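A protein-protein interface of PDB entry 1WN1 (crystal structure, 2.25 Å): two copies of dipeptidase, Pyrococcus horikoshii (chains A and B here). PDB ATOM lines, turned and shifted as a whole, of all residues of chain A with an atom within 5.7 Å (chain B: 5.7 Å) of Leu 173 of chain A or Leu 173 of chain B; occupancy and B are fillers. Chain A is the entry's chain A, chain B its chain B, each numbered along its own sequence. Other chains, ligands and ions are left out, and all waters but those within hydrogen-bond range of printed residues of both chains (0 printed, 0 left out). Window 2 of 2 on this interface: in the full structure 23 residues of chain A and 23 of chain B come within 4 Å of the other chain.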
ATOM      1  N   ALA A 168     -21.855   5.976 -10.207  1.00  0.00           N
ATOM      2  CA  ALA A 168     -20.845   4.993 -10.593  1.00  0.00           C
ATOM      3  C   ALA A 168     -19.793   4.883  -9.490  1.00  0.00           C
ATOM      4  O   ALA A 168     -19.387   3.785  -9.115  1.00  0.00           O
ATOM      5  CB  ALA A 168     -20.175   5.403 -11.908  1.00  0.00           C
ATOM      6  N   LEU A 169     -19.351   6.026  -8.970  1.00  0.00           N
ATOM      7  CA  LEU A 169     -18.347   6.030  -7.913  1.00  0.00           C
ATOM      8  C   LEU A 169     -18.834   5.291  -6.679  1.00  0.00           C
ATOM      9  O   LEU A 169     -18.097   4.480  -6.121  1.00  0.00           O
ATOM     10  CB  LEU A 169     -17.973   7.460  -7.513  1.00  0.00           C
ATOM     11  CG  LEU A 169     -16.924   7.556  -6.392  1.00  0.00           C
ATOM     12  CD1 LEU A 169     -15.684   6.731  -6.777  1.00  0.00           C
ATOM     13  CD2 LEU A 169     -16.537   9.010  -6.165  1.00  0.00           C
ATOM     14  N   LYS A 170     -20.064   5.580  -6.249  1.00  0.00           N
ATOM     15  CA  LYS A 170     -20.635   4.937  -5.059  1.00  0.00           C
ATOM     16  C   LYS A 170     -20.736   3.427  -5.239  1.00  0.00           C
ATOM     17  O   LYS A 170     -20.523   2.668  -4.295  1.00  0.00           O
ATOM     18  CB  LYS A 170     -22.021   5.512  -4.733  1.00  0.00           C
ATOM     19  CG  LYS A 170     -21.989   6.925  -4.139  1.00  0.00           C
ATOM     20  CD  LYS A 170     -23.399   7.423  -3.806  1.00  0.00           C
ATOM     21  CE  LYS A 170     -23.403   8.902  -3.345  1.00  0.00           C
ATOM     22  NZ  LYS A 170     -22.758   9.126  -2.017  1.00  0.00           N
ATOM     23  N   ILE A 171     -21.066   3.004  -6.456  1.00  0.00           N
ATOM     24  CA  ILE A 171     -21.177   1.591  -6.753  1.00  0.00           C
ATOM     25  C   ILE A 171     -19.764   1.030  -6.652  1.00  0.00           C
ATOM     26  O   ILE A 171     -19.546  -0.008  -6.038  1.00  0.00           O
ATOM     27  CB  ILE A 171     -21.775   1.363  -8.164  1.00  0.00           C
ATOM     28  CG1 ILE A 171     -23.260   1.761  -8.164  1.00  0.00           C
ATOM     29  CG2 ILE A 171     -21.606  -0.090  -8.570  1.00  0.00           C
ATOM     30  CD1 ILE A 171     -23.972   1.660  -9.524  1.00  0.00           C
ATOM     31  N   GLU A 172     -18.794   1.748  -7.215  1.00  0.00           N
ATOM     32  CA  GLU A 172     -17.414   1.298  -7.157  1.00  0.00           C
ATOM     33  C   GLU A 172     -16.991   1.075  -5.708  1.00  0.00           C
ATOM     34  O   GLU A 172     -16.525  -0.013  -5.347  1.00  0.00           O
ATOM     35  CB  GLU A 172     -16.466   2.317  -7.807  1.00  0.00           C
ATOM     36  CG  GLU A 172     -14.990   2.122  -7.411  1.00  0.00           C
ATOM     37  CD  GLU A 172     -14.030   3.138  -8.063  1.00  0.00           C
ATOM     38  OE1 GLU A 172     -12.832   3.130  -7.723  1.00  0.00           O
ATOM     39  OE2 GLU A 172     -14.463   3.939  -8.911  1.00  0.00           O
ATOM     40  N   LEU A 173     -17.159   2.107  -4.882  1.00  0.00           N
ATOM     41  CA  LEU A 173     -16.756   2.019  -3.487  1.00  0.00           C
ATOM     42  C   LEU A 173     -17.498   0.916  -2.723  1.00  0.00           C
ATOM     43  O   LEU A 173     -16.883   0.185  -1.963  1.00  0.00           O
ATOM     44  CB  LEU A 173     -16.915   3.384  -2.795  1.00  0.00           C
ATOM     45  CG  LEU A 173     -15.968   4.454  -3.364  1.00  0.00           C
ATOM     46  CD1 LEU A 173     -16.239   5.813  -2.735  1.00  0.00           C
ATOM     47  CD2 LEU A 173     -14.512   4.029  -3.122  1.00  0.00           C
ATOM     48  N   LEU A 174     -18.802   0.767  -2.929  1.00  0.00           N
ATOM     49  CA  LEU A 174     -19.505  -0.276  -2.198  1.00  0.00           C
ATOM     50  C   LEU A 174     -18.960  -1.646  -2.596  1.00  0.00           C
ATOM     51  O   LEU A 174     -18.822  -2.542  -1.762  1.00  0.00           O
ATOM     52  CB  LEU A 174     -21.002  -0.225  -2.470  1.00  0.00           C
ATOM     53  CG  LEU A 174     -21.748  -1.243  -1.600  1.00  0.00           C
ATOM     54  CD1 LEU A 174     -21.559  -0.892  -0.117  1.00  0.00           C
ATOM     55  CD2 LEU A 174     -23.218  -1.255  -1.979  1.00  0.00           C
ATOM     56  N   ILE A 175     -18.639  -1.802  -3.877  1.00  0.00           N
ATOM     57  CA  ILE A 175     -18.106  -3.058  -4.355  1.00  0.00           C
ATOM     58  C   ILE A 175     -16.728  -3.296  -3.746  1.00  0.00           C
ATOM     59  O   ILE A 175     -16.382  -4.425  -3.415  1.00  0.00           O
ATOM     60  CB  ILE A 175     -17.971  -3.072  -5.892  1.00  0.00           C
ATOM     61  CG1 ILE A 175     -19.355  -3.158  -6.537  1.00  0.00           C
ATOM     62  CG2 ILE A 175     -17.091  -4.248  -6.319  1.00  0.00           C
ATOM     63  CD1 ILE A 175     -19.316  -3.183  -8.034  1.00  0.00           C
ATOM     64  N   ARG A 176     -15.934  -2.244  -3.603  1.00  0.00           N
ATOM     65  CA  ARG A 176     -14.607  -2.427  -3.033  1.00  0.00           C
ATOM     66  C   ARG A 176     -14.683  -2.724  -1.544  1.00  0.00           C
ATOM     67  O   ARG A 176     -13.793  -3.341  -0.977  1.00  0.00           O
ATOM     68  CB  ARG A 176     -13.733  -1.211  -3.331  1.00  0.00           C
ATOM     69  CG  ARG A 176     -13.442  -1.123  -4.826  1.00  0.00           C
ATOM     70  CD  ARG A 176     -12.775   0.166  -5.239  1.00  0.00           C
ATOM     71  NE  ARG A 176     -11.396   0.234  -4.771  1.00  0.00           N
ATOM     72  CZ  ARG A 176     -10.553   1.191  -5.120  1.00  0.00           C
ATOM     73  NH1 ARG A 176     -10.961   2.158  -5.939  1.00  0.00           N
ATOM     74  NH2 ARG A 176      -9.309   1.184  -4.658  1.00  0.00           N
ATOM     75  N   GLU A 177     -15.778  -2.310  -0.924  1.00  0.00           N
ATOM     76  CA  GLU A 177     -15.992  -2.561   0.498  1.00  0.00           C
ATOM     77  C   GLU A 177     -16.342  -4.036   0.677  1.00  0.00           C
ATOM     78  O   GLU A 177     -15.725  -4.742   1.462  1.00  0.00           O
ATOM     79  CB  GLU A 177     -17.144  -1.692   1.026  1.00  0.00           C
ATOM     80  CG  GLU A 177     -17.482  -1.875   2.521  1.00  0.00           C
ATOM     81  CD  GLU A 177     -18.618  -0.949   2.997  1.00  0.00           C
ATOM     82  OE1 GLU A 177     -18.487   0.290   2.865  1.00  0.00           O
ATOM     83  OE2 GLU A 177     -19.643  -1.455   3.509  1.00  0.00           O
ATOM     84  N   LEU A 178     -17.329  -4.484  -0.090  1.00  0.00           N
ATOM     85  CA  LEU A 178     -17.848  -5.849  -0.027  1.00  0.00           C
ATOM     86  C   LEU A 178     -17.046  -6.984  -0.647  1.00  0.00           C
ATOM     87  O   LEU A 178     -17.367  -8.144  -0.400  1.00  0.00           O
ATOM     88  CB  LEU A 178     -19.239  -5.890  -0.656  1.00  0.00           C
ATOM     89  CG  LEU A 178     -20.493  -5.523   0.146  1.00  0.00           C
ATOM     90  CD1 LEU A 178     -20.145  -4.905   1.503  1.00  0.00           C
ATOM     91  CD2 LEU A 178     -21.327  -4.570  -0.709  1.00  0.00           C
ATOM     92  N   ALA B 168      -4.848   4.301   2.167  1.00  0.00           N
ATOM     93  CA  ALA B 168      -4.511   4.373   0.761  1.00  0.00           C
ATOM     94  C   ALA B 168      -5.738   4.721  -0.092  1.00  0.00           C
ATOM     95  O   ALA B 168      -5.645   5.499  -1.044  1.00  0.00           O
ATOM     96  CB  ALA B 168      -3.907   3.049   0.295  1.00  0.00           C
ATOM     97  N   LEU B 169      -6.883   4.134   0.230  1.00  0.00           N
ATOM     98  CA  LEU B 169      -8.092   4.410  -0.536  1.00  0.00           C
ATOM     99  C   LEU B 169      -8.533   5.873  -0.343  1.00  0.00           C
ATOM    100  O   LEU B 169      -9.027   6.512  -1.284  1.00  0.00           O
ATOM    101  CB  LEU B 169      -9.203   3.445  -0.118  1.00  0.00           C
ATOM    102  CG  LEU B 169     -10.608   3.731  -0.640  1.00  0.00           C
ATOM    103  CD1 LEU B 169     -10.605   3.700  -2.154  1.00  0.00           C
ATOM    104  CD2 LEU B 169     -11.574   2.699  -0.084  1.00  0.00           C
ATOM    105  N   LYS B 170      -8.352   6.405   0.867  1.00  0.00           N
ATOM    106  CA  LYS B 170      -8.722   7.794   1.111  1.00  0.00           C
ATOM    107  C   LYS B 170      -7.817   8.686   0.276  1.00  0.00           C
ATOM    108  O   LYS B 170      -8.288   9.589  -0.403  1.00  0.00           O
ATOM    109  CB  LYS B 170      -8.607   8.137   2.592  1.00  0.00           C
ATOM    110  CG  LYS B 170      -9.639   7.403   3.440  1.00  0.00           C
ATOM    111  CD  LYS B 170      -9.772   7.990   4.837  1.00  0.00           C
ATOM    112  CE  LYS B 170     -10.953   7.353   5.586  1.00  0.00           C
ATOM    113  NZ  LYS B 170     -11.467   8.199   6.714  1.00  0.00           N
ATOM    114  N   ILE B 171      -6.515   8.423   0.318  1.00  0.00           N
ATOM    115  CA  ILE B 171      -5.559   9.180  -0.479  1.00  0.00           C
ATOM    116  C   ILE B 171      -5.966   9.116  -1.956  1.00  0.00           C
ATOM    117  O   ILE B 171      -6.011  10.132  -2.655  1.00  0.00           O
ATOM    118  CB  ILE B 171      -4.140   8.608  -0.318  1.00  0.00           C
ATOM    119  CG1 ILE B 171      -3.618   8.971   1.072  1.00  0.00           C
ATOM    120  CG2 ILE B 171      -3.228   9.123  -1.415  1.00  0.00           C
ATOM    121  CD1 ILE B 171      -2.263   8.402   1.394  1.00  0.00           C
ATOM    122  N   GLU B 172      -6.276   7.915  -2.419  1.00  0.00           N
ATOM    123  CA  GLU B 172      -6.676   7.724  -3.799  1.00  0.00           C
ATOM    124  C   GLU B 172      -7.915   8.550  -4.163  1.00  0.00           C
ATOM    125  O   GLU B 172      -7.931   9.219  -5.191  1.00  0.00           O
ATOM    126  CB  GLU B 172      -6.947   6.240  -4.060  1.00  0.00           C
ATOM    127  CG  GLU B 172      -7.616   5.964  -5.392  1.00  0.00           C
ATOM    128  CD  GLU B 172      -8.165   4.549  -5.518  1.00  0.00           C
ATOM    129  OE1 GLU B 172      -9.016   4.340  -6.396  1.00  0.00           O
ATOM    130  OE2 GLU B 172      -7.750   3.651  -4.761  1.00  0.00           O
ATOM    131  N   LEU B 173      -8.957   8.500  -3.339  1.00  0.00           N
ATOM    132  CA  LEU B 173     -10.181   9.250  -3.639  1.00  0.00           C
ATOM    133  C   LEU B 173      -9.901  10.757  -3.660  1.00  0.00           C
ATOM    134  O   LEU B 173     -10.425  11.481  -4.503  1.00  0.00           O
ATOM    135  CB  LEU B 173     -11.291   8.915  -2.624  1.00  0.00           C
ATOM    136  CG  LEU B 173     -12.330   7.799  -2.907  1.00  0.00           C
ATOM    137  CD1 LEU B 173     -12.127   7.138  -4.240  1.00  0.00           C
ATOM    138  CD2 LEU B 173     -12.275   6.755  -1.813  1.00  0.00           C
ATOM    139  N   LEU B 174      -9.056  11.221  -2.747  1.00  0.00           N
ATOM    140  CA  LEU B 174      -8.716  12.626  -2.707  1.00  0.00           C
ATOM    141  C   LEU B 174      -8.009  13.016  -4.013  1.00  0.00           C
ATOM    142  O   LEU B 174      -8.353  14.022  -4.640  1.00  0.00           O
ATOM    143  CB  LEU B 174      -7.829  12.919  -1.498  1.00  0.00           C
ATOM    144  CG  LEU B 174      -7.449  14.396  -1.344  1.00  0.00           C
ATOM    145  CD1 LEU B 174      -8.696  15.267  -1.398  1.00  0.00           C
ATOM    146  CD2 LEU B 174      -6.710  14.598  -0.032  1.00  0.00           C
ATOM    147  N   ILE B 175      -7.044  12.202  -4.439  1.00  0.00           N
ATOM    148  CA  ILE B 175      -6.323  12.483  -5.676  1.00  0.00           C
ATOM    149  C   ILE B 175      -7.281  12.532  -6.862  1.00  0.00           C
ATOM    150  O   ILE B 175      -7.185  13.405  -7.712  1.00  0.00           O
ATOM    151  CB  ILE B 175      -5.212  11.431  -5.935  1.00  0.00           C
ATOM    152  CG1 ILE B 175      -4.092  11.624  -4.906  1.00  0.00           C
ATOM    153  CG2 ILE B 175      -4.642  11.580  -7.346  1.00  0.00           C
ATOM    154  CD1 ILE B 175      -3.036  10.535  -4.910  1.00  0.00           C
ATOM    155  N   ARG B 176      -8.213  11.591  -6.911  1.00  0.00           N
ATOM    156  CA  ARG B 176      -9.183  11.549  -7.999  1.00  0.00           C
ATOM    157  C   ARG B 176     -10.095  12.768  -7.924  1.00  0.00           C
ATOM    158  O   ARG B 176     -10.623  13.214  -8.934  1.00  0.00           O
ATOM    159  CB  ARG B 176      -9.978  10.238  -7.941  1.00  0.00           C
ATOM    160  CG  ARG B 176      -9.130   9.054  -8.411  1.00  0.00           C
ATOM    161  CD  ARG B 176      -9.736   7.690  -8.089  1.00  0.00           C
ATOM    162  NE  ARG B 176     -10.996   7.455  -8.782  1.00  0.00           N
ATOM    163  CZ  ARG B 176     -11.757   6.381  -8.594  1.00  0.00           C
ATOM    164  NH1 ARG B 176     -11.375   5.445  -7.737  1.00  0.00           N
ATOM    165  NH2 ARG B 176     -12.907   6.255  -9.245  1.00  0.00           N
ATOM    166  N   GLU B 177     -10.252  13.317  -6.724  1.00  0.00           N
ATOM    167  CA  GLU B 177     -11.068  14.511  -6.532  1.00  0.00           C
ATOM    168  C   GLU B 177     -10.334  15.748  -7.053  1.00  0.00           C
ATOM    169  O   GLU B 177     -10.863  16.505  -7.856  1.00  0.00           O
ATOM    170  CB  GLU B 177     -11.370  14.725  -5.044  1.00  0.00           C
ATOM    171  CG  GLU B 177     -12.849  14.654  -4.661  1.00  0.00           C
ATOM    172  CD  GLU B 177     -13.074  14.607  -3.139  1.00  0.00           C
ATOM    173  OE1 GLU B 177     -13.915  13.786  -2.694  1.00  0.00           O
ATOM    174  OE2 GLU B 177     -12.421  15.390  -2.394  1.00  0.00           O
ATOM    175  N   LEU B 178      -9.106  15.939  -6.585  1.00  0.00           N
ATOM    176  CA  LEU B 178      -8.296  17.099  -6.953  1.00  0.00           C
ATOM    177  C   LEU B 178      -7.643  17.105  -8.339  1.00  0.00           C
ATOM    178  O   LEU B 178      -7.242  18.159  -8.829  1.00  0.00           O
ATOM    179  CB  LEU B 178      -7.201  17.292  -5.901  1.00  0.00           C
ATOM    180  CG  LEU B 178      -7.569  17.933  -4.555  1.00  0.00           C
ATOM    181  CD1 LEU B 178      -8.975  17.547  -4.144  1.00  0.00           C
ATOM    182  CD2 LEU B 178      -6.543  17.509  -3.495  1.00  0.00           C
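Leu 169 of chain A touches Arg 176 of chain B, and with the chains exchanged Arg 176 of chain A touches Leu 169 of chain B.
Glu 172 of chain A touches Arg 176 of chain B, and with the chains exchanged Arg 176 of chain A touches Glu 172 of chain B.
Leu 173 of chain A touches its own counterpart, Leu 173 of chain B.
Arg 176 of chain B touches its own counterpart, Arg 176 of chain A.
Of the 6 pairs that touch across the chains among the printed residues, 6 have their exchanged pair printed and touching as well.
OE2 of Glu 172 of chain B lies within salt-bridge range of NH2 of Arg 176 of chain A (2.9 Å).
The guanidinium group of Arg 176 of chain B is in salt-bridge range of the side-chain carboxylate of Glu 172 of chain A, 2.7 Å away.
The side-chain carboxylate of Glu 172 of chain A is in salt-bridge range of the guanidinium group of Arg 176 of chain A, 2.8 Å away.
The guanidinium group (NH1) of Arg 176 of chain B is in salt-bridge range of the side-chain carboxylate (OE1) of Glu 172 of chain B (2.9 Å).
Of the 11 printed residues of chain B, 4 touch a printed residue of chain A.
Along chain B the printed residues that touch a printed residue of chain A span positions 169 to 176.
Printed residues of chain A that touch a printed residue of chain B: Leu 169, Glu 172, Leu 173 and Arg 176.
Hydrophobic or aromatic side chains of chain A that line the printed part of chain B: Leu 169 and Leu 173.
Among the printed residues, Asp or Glu carboxylates within 4 Å of a Lys or Arg side-chain nitrogen of the other chain: Glu 172 of chain A with Arg 176 of chain B and Arg 176 of chain A with Glu 172 of chain B.
Of chain B, only Leu 173 (3.8 Å) comes within 4 Å of Leu 173 of chain A.
Leu 173 of chain B touches one residue of chain A.
Printed residues of chain A within 4 Å of Glu 172 of chain B: Arg 176.
Of the printed residues of chain A, Arg 176 of chain B touches Leu 169, Glu 172 and Arg 176.
Of the printed residues of chain B, Leu 169 of chain A touches Arg 176.
The nearest residue of chain A that does not touch Leu 173 of chain B is Leu 169 of chain A (4.4 Å).
NH2 of Arg 176 of chain B touches CD1 of Leu 169 of chain A, 3.7 Å away.
CD2 of Leu 173 of chain A touches CD2 of Leu 173 of chain B, at 3.8 Å.
CD1 of Leu 169 of chain B touches NH2 of Arg 176 of chain A, at 3.8 Å.
Arg 176 of chain B touches Arg 176 of chain A (NH1 to NH1, 3.8 Å).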
